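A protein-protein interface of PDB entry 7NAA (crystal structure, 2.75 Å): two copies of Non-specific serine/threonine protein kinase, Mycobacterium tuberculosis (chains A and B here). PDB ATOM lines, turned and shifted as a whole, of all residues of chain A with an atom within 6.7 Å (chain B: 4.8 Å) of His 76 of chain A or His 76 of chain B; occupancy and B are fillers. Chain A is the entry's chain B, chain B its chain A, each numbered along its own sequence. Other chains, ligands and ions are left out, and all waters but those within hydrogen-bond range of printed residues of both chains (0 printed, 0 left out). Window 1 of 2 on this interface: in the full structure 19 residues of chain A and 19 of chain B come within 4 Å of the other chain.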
ATOM      1  N   HIS A  31       9.502 -25.664  -6.568  1.00  0.00           N
ATOM      2  CA  HIS A  31       8.387 -24.701  -6.379  1.00  0.00           C
ATOM      3  C   HIS A  31       7.638 -24.548  -7.700  1.00  0.00           C
ATOM      4  O   HIS A  31       8.247 -24.549  -8.766  1.00  0.00           O
ATOM      5  CB  HIS A  31       8.926 -23.362  -5.838  1.00  0.00           C
ATOM      6  CG  HIS A  31       7.878 -22.440  -5.306  1.00  0.00           C
ATOM      7  ND1 HIS A  31       7.107 -21.664  -6.128  1.00  0.00           N
ATOM      8  CD2 HIS A  31       7.493 -22.146  -4.048  1.00  0.00           C
ATOM      9  CE1 HIS A  31       6.279 -20.949  -5.403  1.00  0.00           C
ATOM     10  NE2 HIS A  31       6.492 -21.223  -4.122  1.00  0.00           N
ATOM     11  N   LEU A  34       8.579 -20.319  -8.743  1.00  0.00           N
ATOM     12  CA  LEU A  34       9.988 -19.862  -8.595  1.00  0.00           C
ATOM     13  C   LEU A  34      10.933 -21.000  -8.962  1.00  0.00           C
ATOM     14  O   LEU A  34      10.677 -22.149  -8.614  1.00  0.00           O
ATOM     15  CB  LEU A  34      10.203 -19.405  -7.149  1.00  0.00           C
ATOM     16  CG  LEU A  34       9.276 -18.290  -6.675  1.00  0.00           C
ATOM     17  CD1 LEU A  34       9.507 -17.991  -5.202  1.00  0.00           C
ATOM     18  CD2 LEU A  34       9.482 -17.023  -7.494  1.00  0.00           C
ATOM     19  N   ARG A  36      13.494 -22.756  -7.798  1.00  0.00           N
ATOM     20  CA  ARG A  36      14.284 -23.171  -6.610  1.00  0.00           C
ATOM     21  C   ARG A  36      13.618 -24.393  -5.974  1.00  0.00           C
ATOM     22  O   ARG A  36      12.446 -24.672  -6.298  1.00  0.00           O
ATOM     23  CB  ARG A  36      14.371 -22.033  -5.590  1.00  0.00           C
ATOM     24  CG  ARG A  36      13.012 -21.624  -5.046  1.00  0.00           C
ATOM     25  CD  ARG A  36      13.033 -20.837  -3.760  1.00  0.00           C
ATOM     26  NE  ARG A  36      11.677 -20.801  -3.222  1.00  0.00           N
ATOM     27  CZ  ARG A  36      11.135 -19.782  -2.561  1.00  0.00           C
ATOM     28  NH1 ARG A  36      11.825 -18.671  -2.345  1.00  0.00           N
ATOM     29  NH2 ARG A  36       9.897 -19.891  -2.101  1.00  0.00           N
ATOM     30  N   ASP A  38      12.304 -26.286  -2.451  1.00  0.00           N
ATOM     31  CA  ASP A  38      11.755 -26.031  -1.096  1.00  0.00           C
ATOM     32  C   ASP A  38      11.562 -27.366  -0.363  1.00  0.00           C
ATOM     33  O   ASP A  38      11.563 -28.429  -1.032  1.00  0.00           O
ATOM     34  CB  ASP A  38      10.425 -25.284  -1.176  1.00  0.00           C
ATOM     35  CG  ASP A  38      10.526 -23.867  -1.713  1.00  0.00           C
ATOM     36  OD1 ASP A  38      11.657 -23.342  -1.837  1.00  0.00           O
ATOM     37  OD2 ASP A  38       9.469 -23.298  -2.005  1.00  0.00           O
ATOM     38  N   TRP A  68      11.321 -14.802  12.539  1.00  0.00           N
ATOM     39  CA  TRP A  68      12.224 -14.289  11.473  1.00  0.00           C
ATOM     40  C   TRP A  68      13.637 -14.201  12.061  1.00  0.00           C
ATOM     41  O   TRP A  68      13.957 -13.213  12.757  1.00  0.00           O
ATOM     42  CB  TRP A  68      11.685 -12.945  10.946  1.00  0.00           C
ATOM     43  CG  TRP A  68      12.423 -12.342   9.787  1.00  0.00           C
ATOM     44  CD1 TRP A  68      12.350 -12.729   8.484  1.00  0.00           C
ATOM     45  CD2 TRP A  68      13.310 -11.206   9.812  1.00  0.00           C
ATOM     46  NE1 TRP A  68      13.144 -11.939   7.699  1.00  0.00           N
ATOM     47  CE2 TRP A  68      13.757 -11.002   8.488  1.00  0.00           C
ATOM     48  CE3 TRP A  68      13.795 -10.370  10.826  1.00  0.00           C
ATOM     49  CZ2 TRP A  68      14.657  -9.985   8.154  1.00  0.00           C
ATOM     50  CZ3 TRP A  68      14.701  -9.387  10.500  1.00  0.00           C
ATOM     51  CH2 TRP A  68      15.124  -9.199   9.181  1.00  0.00           C
ATOM     52  N   ALA A  74      12.725 -20.767   7.443  1.00  0.00           N
ATOM     53  CA  ALA A  74      11.614 -19.840   7.133  1.00  0.00           C
ATOM     54  C   ALA A  74      10.453 -20.609   6.503  1.00  0.00           C
ATOM     55  O   ALA A  74      10.730 -21.480   5.667  1.00  0.00           O
ATOM     56  CB  ALA A  74      12.105 -18.780   6.190  1.00  0.00           C
ATOM     57  N   VAL A  75       9.217 -20.276   6.864  1.00  0.00           N
ATOM     58  CA  VAL A  75       7.978 -20.762   6.186  1.00  0.00           C
ATOM     59  C   VAL A  75       7.566 -19.732   5.131  1.00  0.00           C
ATOM     60  O   VAL A  75       7.479 -18.546   5.462  1.00  0.00           O
ATOM     61  CB  VAL A  75       6.829 -20.974   7.186  1.00  0.00           C
ATOM     62  CG1 VAL A  75       5.525 -21.320   6.466  1.00  0.00           C
ATOM     63  CG2 VAL A  75       7.168 -22.019   8.238  1.00  0.00           C
ATOM     64  N   HIS A  76       7.308 -20.179   3.905  1.00  0.00           N
ATOM     65  CA  HIS A  76       6.830 -19.332   2.783  1.00  0.00           C
ATOM     66  C   HIS A  76       5.302 -19.293   2.780  1.00  0.00           C
ATOM     67  O   HIS A  76       4.772 -18.203   2.642  1.00  0.00           O
ATOM     68  CB  HIS A  76       7.402 -19.833   1.456  1.00  0.00           C
ATOM     69  CG  HIS A  76       8.892 -19.786   1.406  1.00  0.00           C
ATOM     70  ND1 HIS A  76       9.590 -18.646   1.753  1.00  0.00           N
ATOM     71  CD2 HIS A  76       9.816 -20.718   1.090  1.00  0.00           C
ATOM     72  CE1 HIS A  76      10.881 -18.861   1.621  1.00  0.00           C
ATOM     73  NE2 HIS A  76      11.052 -20.124   1.214  1.00  0.00           N
ATOM     74  N   ASP A  77       4.632 -20.433   2.946  1.00  0.00           N
ATOM     75  CA  ASP A  77       3.160 -20.565   2.753  1.00  0.00           C
ATOM     76  C   ASP A  77       2.646 -21.883   3.367  1.00  0.00           C
ATOM     77  O   ASP A  77       3.448 -22.802   3.587  1.00  0.00           O
ATOM     78  CB  ASP A  77       2.839 -20.472   1.259  1.00  0.00           C
ATOM     79  CG  ASP A  77       1.489 -19.880   0.907  1.00  0.00           C
ATOM     80  OD1 ASP A  77       0.680 -19.670   1.827  1.00  0.00           O
ATOM     81  OD2 ASP A  77       1.235 -19.716  -0.301  1.00  0.00           O
ATOM     82  N   ARG A  78       1.341 -21.949   3.638  1.00  0.00           N
ATOM     83  CA  ARG A  78       0.585 -23.143   4.112  1.00  0.00           C
ATOM     84  C   ARG A  78      -0.622 -23.310   3.183  1.00  0.00           C
ATOM     85  O   ARG A  78      -0.957 -22.329   2.482  1.00  0.00           O
ATOM     86  CB  ARG A  78       0.132 -22.954   5.569  1.00  0.00           C
ATOM     87  N   TRP A  86      -0.437 -28.896   3.829  1.00  0.00           N
ATOM     88  CA  TRP A  86       0.990 -28.762   3.423  1.00  0.00           C
ATOM     89  C   TRP A  86       1.584 -27.450   3.951  1.00  0.00           C
ATOM     90  O   TRP A  86       0.842 -26.459   4.050  1.00  0.00           O
ATOM     91  CB  TRP A  86       1.144 -28.877   1.899  1.00  0.00           C
ATOM     92  CG  TRP A  86       0.366 -27.879   1.098  1.00  0.00           C
ATOM     93  CD1 TRP A  86      -0.871 -28.049   0.547  1.00  0.00           C
ATOM     94  CD2 TRP A  86       0.795 -26.565   0.712  1.00  0.00           C
ATOM     95  NE1 TRP A  86      -1.244 -26.931  -0.150  1.00  0.00           N
ATOM     96  CE2 TRP A  86      -0.240 -26.005  -0.068  1.00  0.00           C
ATOM     97  CE3 TRP A  86       1.944 -25.804   0.953  1.00  0.00           C
ATOM     98  CZ2 TRP A  86      -0.157 -24.722  -0.602  1.00  0.00           C
ATOM     99  CZ3 TRP A  86       2.026 -24.540   0.420  1.00  0.00           C
ATOM    100  CH2 TRP A  86       0.988 -24.007  -0.345  1.00  0.00           C
ATOM    101  N   ILE A  87       2.884 -27.471   4.257  1.00  0.00           N
ATOM    102  CA  ILE A  87       3.703 -26.289   4.650  1.00  0.00           C
ATOM    103  C   ILE A  87       4.911 -26.211   3.711  1.00  0.00           C
ATOM    104  O   ILE A  87       5.728 -27.152   3.720  1.00  0.00           O
ATOM    105  CB  ILE A  87       4.141 -26.394   6.121  1.00  0.00           C
ATOM    106  CG1 ILE A  87       2.944 -26.619   7.049  1.00  0.00           C
ATOM    107  CG2 ILE A  87       4.973 -25.177   6.525  1.00  0.00           C
ATOM    108  CD1 ILE A  87       3.332 -27.010   8.457  1.00  0.00           C
ATOM    109  N   ASP A  88       4.998 -25.132   2.927  1.00  0.00           N
ATOM    110  CA  ASP A  88       6.157 -24.796   2.057  1.00  0.00           C
ATOM    111  C   ASP A  88       7.153 -24.014   2.914  1.00  0.00           C
ATOM    112  O   ASP A  88       6.750 -22.996   3.480  1.00  0.00           O
ATOM    113  CB  ASP A  88       5.691 -24.034   0.810  1.00  0.00           C
ATOM    114  CG  ASP A  88       6.798 -23.473  -0.060  1.00  0.00           C
ATOM    115  OD1 ASP A  88       7.871 -24.091  -0.111  1.00  0.00           O
ATOM    116  OD2 ASP A  88       6.575 -22.407  -0.678  1.00  0.00           O
ATOM    117  N   MET A  89       8.388 -24.499   3.042  1.00  0.00           N
ATOM    118  CA  MET A  89       9.451 -23.836   3.852  1.00  0.00           C
ATOM    119  C   MET A  89      10.797 -23.927   3.124  1.00  0.00           C
ATOM    120  O   MET A  89      10.893 -24.694   2.162  1.00  0.00           O
ATOM    121  CB  MET A  89       9.563 -24.456   5.256  1.00  0.00           C
ATOM    122  CG  MET A  89       9.903 -25.929   5.271  1.00  0.00           C
ATOM    123  SD  MET A  89       9.621 -26.711   6.875  1.00  0.00           S
ATOM    124  CE  MET A  89       9.153 -28.368   6.378  1.00  0.00           C
ATOM    125  N   ASP A  90      11.769 -23.119   3.544  1.00  0.00           N
ATOM    126  CA  ASP A  90      13.158 -23.128   3.025  1.00  0.00           C
ATOM    127  C   ASP A  90      13.690 -24.557   3.019  1.00  0.00           C
ATOM    128  O   ASP A  90      13.420 -25.274   3.984  1.00  0.00           O
ATOM    129  CB  ASP A  90      14.105 -22.314   3.903  1.00  0.00           C
ATOM    130  CG  ASP A  90      14.141 -20.834   3.607  1.00  0.00           C
ATOM    131  OD1 ASP A  90      13.852 -20.468   2.455  1.00  0.00           O
ATOM    132  OD2 ASP A  90      14.495 -20.078   4.544  1.00  0.00           O
ATOM    133  N   PHE A  91      14.417 -24.933   1.969  1.00  0.00           N
ATOM    134  CA  PHE A  91      15.218 -26.175   1.910  1.00  0.00           C
ATOM    135  C   PHE A  91      16.664 -25.828   2.254  1.00  0.00           C
ATOM    136  O   PHE A  91      17.269 -25.021   1.536  1.00  0.00           O
ATOM    137  CB  PHE A  91      15.148 -26.813   0.522  1.00  0.00           C
ATOM    138  CG  PHE A  91      16.185 -27.878   0.285  1.00  0.00           C
ATOM    139  CD1 PHE A  91      16.215 -29.016   1.071  1.00  0.00           C
ATOM    140  CD2 PHE A  91      17.138 -27.735  -0.708  1.00  0.00           C
ATOM    141  CE1 PHE A  91      17.170 -30.000   0.861  1.00  0.00           C
ATOM    142  CE2 PHE A  91      18.093 -28.717  -0.918  1.00  0.00           C
ATOM    143  CZ  PHE A  91      18.109 -29.848  -0.132  1.00  0.00           C
ATOM    144  N   HIS B  31      -0.520 -11.222   5.150  1.00  0.00           N
ATOM    145  CA  HIS B  31      -0.515 -12.442   4.293  1.00  0.00           C
ATOM    146  C   HIS B  31      -1.904 -13.066   4.339  1.00  0.00           C
ATOM    147  O   HIS B  31      -2.548 -13.056   5.384  1.00  0.00           O
ATOM    148  CB  HIS B  31       0.599 -13.407   4.740  1.00  0.00           C
ATOM    149  CG  HIS B  31       0.887 -14.525   3.794  1.00  0.00           C
ATOM    150  ND1 HIS B  31       0.095 -15.653   3.713  1.00  0.00           N
ATOM    151  CD2 HIS B  31       1.893 -14.708   2.907  1.00  0.00           C
ATOM    152  CE1 HIS B  31       0.586 -16.470   2.802  1.00  0.00           C
ATOM    153  NE2 HIS B  31       1.714 -15.924   2.309  1.00  0.00           N
ATOM    154  N   LEU B  34      -1.060 -16.984   6.470  1.00  0.00           N
ATOM    155  CA  LEU B  34      -0.197 -16.904   7.679  1.00  0.00           C
ATOM    156  C   LEU B  34      -0.502 -15.605   8.419  1.00  0.00           C
ATOM    157  O   LEU B  34      -0.674 -14.560   7.798  1.00  0.00           O
ATOM    158  CB  LEU B  34       1.276 -16.965   7.266  1.00  0.00           C
ATOM    159  CG  LEU B  34       1.666 -18.180   6.427  1.00  0.00           C
ATOM    160  CD1 LEU B  34       3.088 -18.058   5.910  1.00  0.00           C
ATOM    161  CD2 LEU B  34       1.503 -19.460   7.229  1.00  0.00           C
ATOM    162  N   ARG B  36       1.079 -12.982   9.669  1.00  0.00           N
ATOM    163  CA  ARG B  36       2.278 -12.109   9.674  1.00  0.00           C
ATOM    164  C   ARG B  36       2.130 -11.049   8.581  1.00  0.00           C
ATOM    165  O   ARG B  36       1.249 -11.195   7.727  1.00  0.00           O
ATOM    166  CB  ARG B  36       3.538 -12.939   9.446  1.00  0.00           C
ATOM    167  CG  ARG B  36       3.567 -13.618   8.087  1.00  0.00           C
ATOM    168  CD  ARG B  36       4.939 -14.107   7.650  1.00  0.00           C
ATOM    169  NE  ARG B  36       4.872 -14.457   6.238  1.00  0.00           N
ATOM    170  CZ  ARG B  36       5.532 -15.447   5.645  1.00  0.00           C
ATOM    171  NH1 ARG B  36       6.354 -16.225   6.333  1.00  0.00           N
ATOM    172  NH2 ARG B  36       5.351 -15.657   4.349  1.00  0.00           N
ATOM    173  N   ASP B  38       3.904  -9.044   5.359  1.00  0.00           N
ATOM    174  CA  ASP B  38       4.877  -9.187   4.251  1.00  0.00           C
ATOM    175  C   ASP B  38       4.990  -7.867   3.485  1.00  0.00           C
ATOM    176  O   ASP B  38       4.106  -7.004   3.632  1.00  0.00           O
ATOM    177  CB  ASP B  38       4.462 -10.320   3.307  1.00  0.00           C
ATOM    178  CG  ASP B  38       4.581 -11.709   3.924  1.00  0.00           C
ATOM    179  OD1 ASP B  38       5.175 -11.846   5.024  1.00  0.00           O
ATOM    180  OD2 ASP B  38       4.111 -12.643   3.285  1.00  0.00           O
ATOM    181  N   ALA B  74      14.248 -12.156   1.762  1.00  0.00           N
ATOM    182  CA  ALA B  74      13.758 -13.416   1.148  1.00  0.00           C
ATOM    183  C   ALA B  74      12.485 -13.174   0.339  1.00  0.00           C
ATOM    184  O   ALA B  74      11.625 -12.448   0.836  1.00  0.00           O
ATOM    185  CB  ALA B  74      13.483 -14.433   2.221  1.00  0.00           C
ATOM    186  N   VAL B  75      12.370 -13.780  -0.842  1.00  0.00           N
ATOM    187  CA  VAL B  75      11.112 -13.853  -1.636  1.00  0.00           C
ATOM    188  C   VAL B  75      10.420 -15.174  -1.292  1.00  0.00           C
ATOM    189  O   VAL B  75      11.075 -16.226  -1.353  1.00  0.00           O
ATOM    190  CB  VAL B  75      11.372 -13.742  -3.145  1.00  0.00           C
ATOM    191  CG1 VAL B  75      10.131 -14.048  -3.960  1.00  0.00           C
ATOM    192  CG2 VAL B  75      11.936 -12.383  -3.519  1.00  0.00           C
ATOM    193  N   HIS B  76       9.132 -15.110  -0.968  1.00  0.00           N
ATOM    194  CA  HIS B  76       8.277 -16.284  -0.666  1.00  0.00           C
ATOM    195  C   HIS B  76       7.649 -16.797  -1.965  1.00  0.00           C
ATOM    196  O   HIS B  76       7.684 -18.013  -2.177  1.00  0.00           O
ATOM    197  CB  HIS B  76       7.230 -15.907   0.390  1.00  0.00           C
ATOM    198  CG  HIS B  76       7.841 -15.494   1.686  1.00  0.00           C
ATOM    199  ND1 HIS B  76       8.808 -16.267   2.308  1.00  0.00           N
ATOM    200  CD2 HIS B  76       7.695 -14.394   2.450  1.00  0.00           C
ATOM    201  CE1 HIS B  76       9.201 -15.687   3.421  1.00  0.00           C
ATOM    202  NE2 HIS B  76       8.540 -14.536   3.527  1.00  0.00           N
ATOM    203  N   ASP B  77       7.108 -15.902  -2.801  1.00  0.00           N
ATOM    204  CA  ASP B  77       6.274 -16.270  -3.975  1.00  0.00           C
ATOM    205  C   ASP B  77       6.152 -15.081  -4.947  1.00  0.00           C
ATOM    206  O   ASP B  77       6.358 -13.933  -4.531  1.00  0.00           O
ATOM    207  CB  ASP B  77       4.905 -16.754  -3.491  1.00  0.00           C
ATOM    208  CG  ASP B  77       4.228 -17.789  -4.371  1.00  0.00           C
ATOM    209  OD1 ASP B  77       4.749 -18.072  -5.477  1.00  0.00           O
ATOM    210  OD2 ASP B  77       3.145 -18.256  -3.972  1.00  0.00           O
ATOM    211  N   ASP B  88       5.698 -11.415  -3.304  1.00  0.00           N
ATOM    212  CA  ASP B  88       5.562 -11.533  -1.825  1.00  0.00           C
ATOM    213  C   ASP B  88       6.965 -11.774  -1.262  1.00  0.00           C
ATOM    214  O   ASP B  88       7.604 -12.750  -1.705  1.00  0.00           O
ATOM    215  CB  ASP B  88       4.571 -12.647  -1.462  1.00  0.00           C
ATOM    216  CG  ASP B  88       4.507 -12.993   0.023  1.00  0.00           C
ATOM    217  OD1 ASP B  88       4.728 -12.092   0.850  1.00  0.00           O
ATOM    218  OD2 ASP B  88       4.235 -14.170   0.348  1.00  0.00           O
ATOM    219  N   MET B  89       7.436 -10.898  -0.370  1.00  0.00           N
ATOM    220  CA  MET B  89       8.784 -11.015   0.245  1.00  0.00           C
ATOM    221  C   MET B  89       8.710 -10.658   1.733  1.00  0.00           C
ATOM    222  O   MET B  89       7.696 -10.097   2.155  1.00  0.00           O
ATOM    223  CB  MET B  89       9.815 -10.131  -0.473  1.00  0.00           C
ATOM    224  CG  MET B  89       9.512  -8.655  -0.449  1.00  0.00           C
ATOM    225  SD  MET B  89      10.602  -7.684  -1.515  1.00  0.00           S
ATOM    226  CE  MET B  89       9.498  -6.336  -1.923  1.00  0.00           C
ATOM    227  N   ASP B  90       9.741 -11.026   2.492  1.00  0.00           N
ATOM    228  CA  ASP B  90       9.899 -10.676   3.927  1.00  0.00           C
ATOM    229  C   ASP B  90       9.659  -9.180   4.117  1.00  0.00           C
ATOM    230  O   ASP B  90      10.141  -8.422   3.289  1.00  0.00           O
ATOM    231  CB  ASP B  90      11.316 -10.962   4.423  1.00  0.00           C
ATOM    232  CG  ASP B  90      11.559 -12.378   4.870  1.00  0.00           C
ATOM    233  OD1 ASP B  90      10.570 -13.039   5.253  1.00  0.00           O
ATOM    234  OD2 ASP B  90      12.750 -12.775   4.840  1.00  0.00           O
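NE2 of His 76 of chain A lies within hydrogen-bond range of OD1 of Asp 90 of chain A (3.1 Å).
The backbone carbonyl oxygen (O) of Arg 36 of chain B sits at hydrogen-bond distance from the backbone NH (N) of His 31 of chain B.
N of His 76 of chain A lies within hydrogen-bond range of O of Asp 88 of chain A.
ND1 of His 31 of chain B lies within hydrogen-bond range of N of Leu 34 of chain B (3.3 Å).
The guanidinium group (NE) of Arg 36 of chain A lies within salt-bridge range of the side-chain carboxylate (OD1) of Asp 38 of chain A (2.9 Å).
N of Asp 88 of chain B is in hydrogen-bond range of O of Asp 77 of chain B (2.9 Å).
His 76 of chain A touches just these residues of chain B: His 31, Leu 34, Arg 36, Val 75 and His 76.
His 76 of chain B touches five residues of chain A.
Of the printed residues of chain A, Asp 90 of chain B touches Trp 68.
Of the printed residues of chain B, Arg 36 of chain A touches Val 75 (2.7 Å) and His 76 (2.9 Å).
Met 89 of chain B touches none of the printed residues of chain A.
The nearest printed residue of chain B that does not touch Trp 68 of chain A is Ala 74 of chain B (6.0 Å).
Of the 11 printed residues of chain B, 7 touch a printed residue of chain A.
Of the 16 printed residues of chain A, 7 touch a printed residue of chain B.
Printed residues of chain A that touch a printed residue of chain B: His 31, Leu 34, Arg 36, Trp 68, Val 75, His 76 and Asp 77.
Hydrophobic or aromatic side chains of chain A that line the printed part of chain B: His 31, Leu 34, Trp 68 and His 76.
Among the printed residues, 15 pairs touch across the chains.
His 31 of chain A touches His 76 of chain B, and with the chains exchanged His 76 of chain A touches His 31 of chain B.
His 31 of chain A touches Asp 77 of chain B, and with the chains exchanged Asp 77 of chain A touches His 31 of chain B.
Leu 34 of chain A touches Asp 77 of chain B, but with the chains exchanged Asp 77 of chain A does not touch Leu 34 of chain B (4.03 Å).
Arg 36 of chain A touches His 76 of chain B, and with the chains exchanged His 76 of chain A touches Arg 36 of chain B.
11 positions are printed for both chains.
Among the printed residues, merely in contact across the chains: His 31 of chain A with His 76 of chain B, His 31 of chain A with Asp 77 of chain B, Leu 34 of chain A with His 76 of chain B, Leu 34 of chain A with Asp 77 of chain B, Val 75 of chain A with His 76 of chain B, His 76 of chain A with His 31 of chain B, His 76 of chain A with Leu 34 of chain B, His 76 of chain A with Val 75 of chain B and Asp 77 of chain A with His 31 of chain B.
The guanidinium group (NH2) of Arg 36 of chain B is in hydrogen-bond range of the backbone carbonyl oxygen (O) of His 76 of chain A (3.1 Å).
A ring nitrogen (ND1) of His 76 of chain A sits at hydrogen-bond distance from a ring nitrogen (ND1) of His 76 of chain B (2.6 Å).
NH1 of Arg 36 of chain B is in hydrogen-bond range of O of Val 75 of chain A.
The backbone carbonyl oxygen (O) of His 76 of chain B lies within hydrogen-bond range of the guanidinium group (NH2) of Arg 36 of chain A.
The indole nitrogen (NE1) of Trp 68 of chain A lies within hydrogen-bond range of the side-chain carboxylate (OD2) of Asp 90 of chain B.
NH1 of Arg 36 of chain A is in hydrogen-bond range of O of Val 75 of chain B (2.7 Å).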
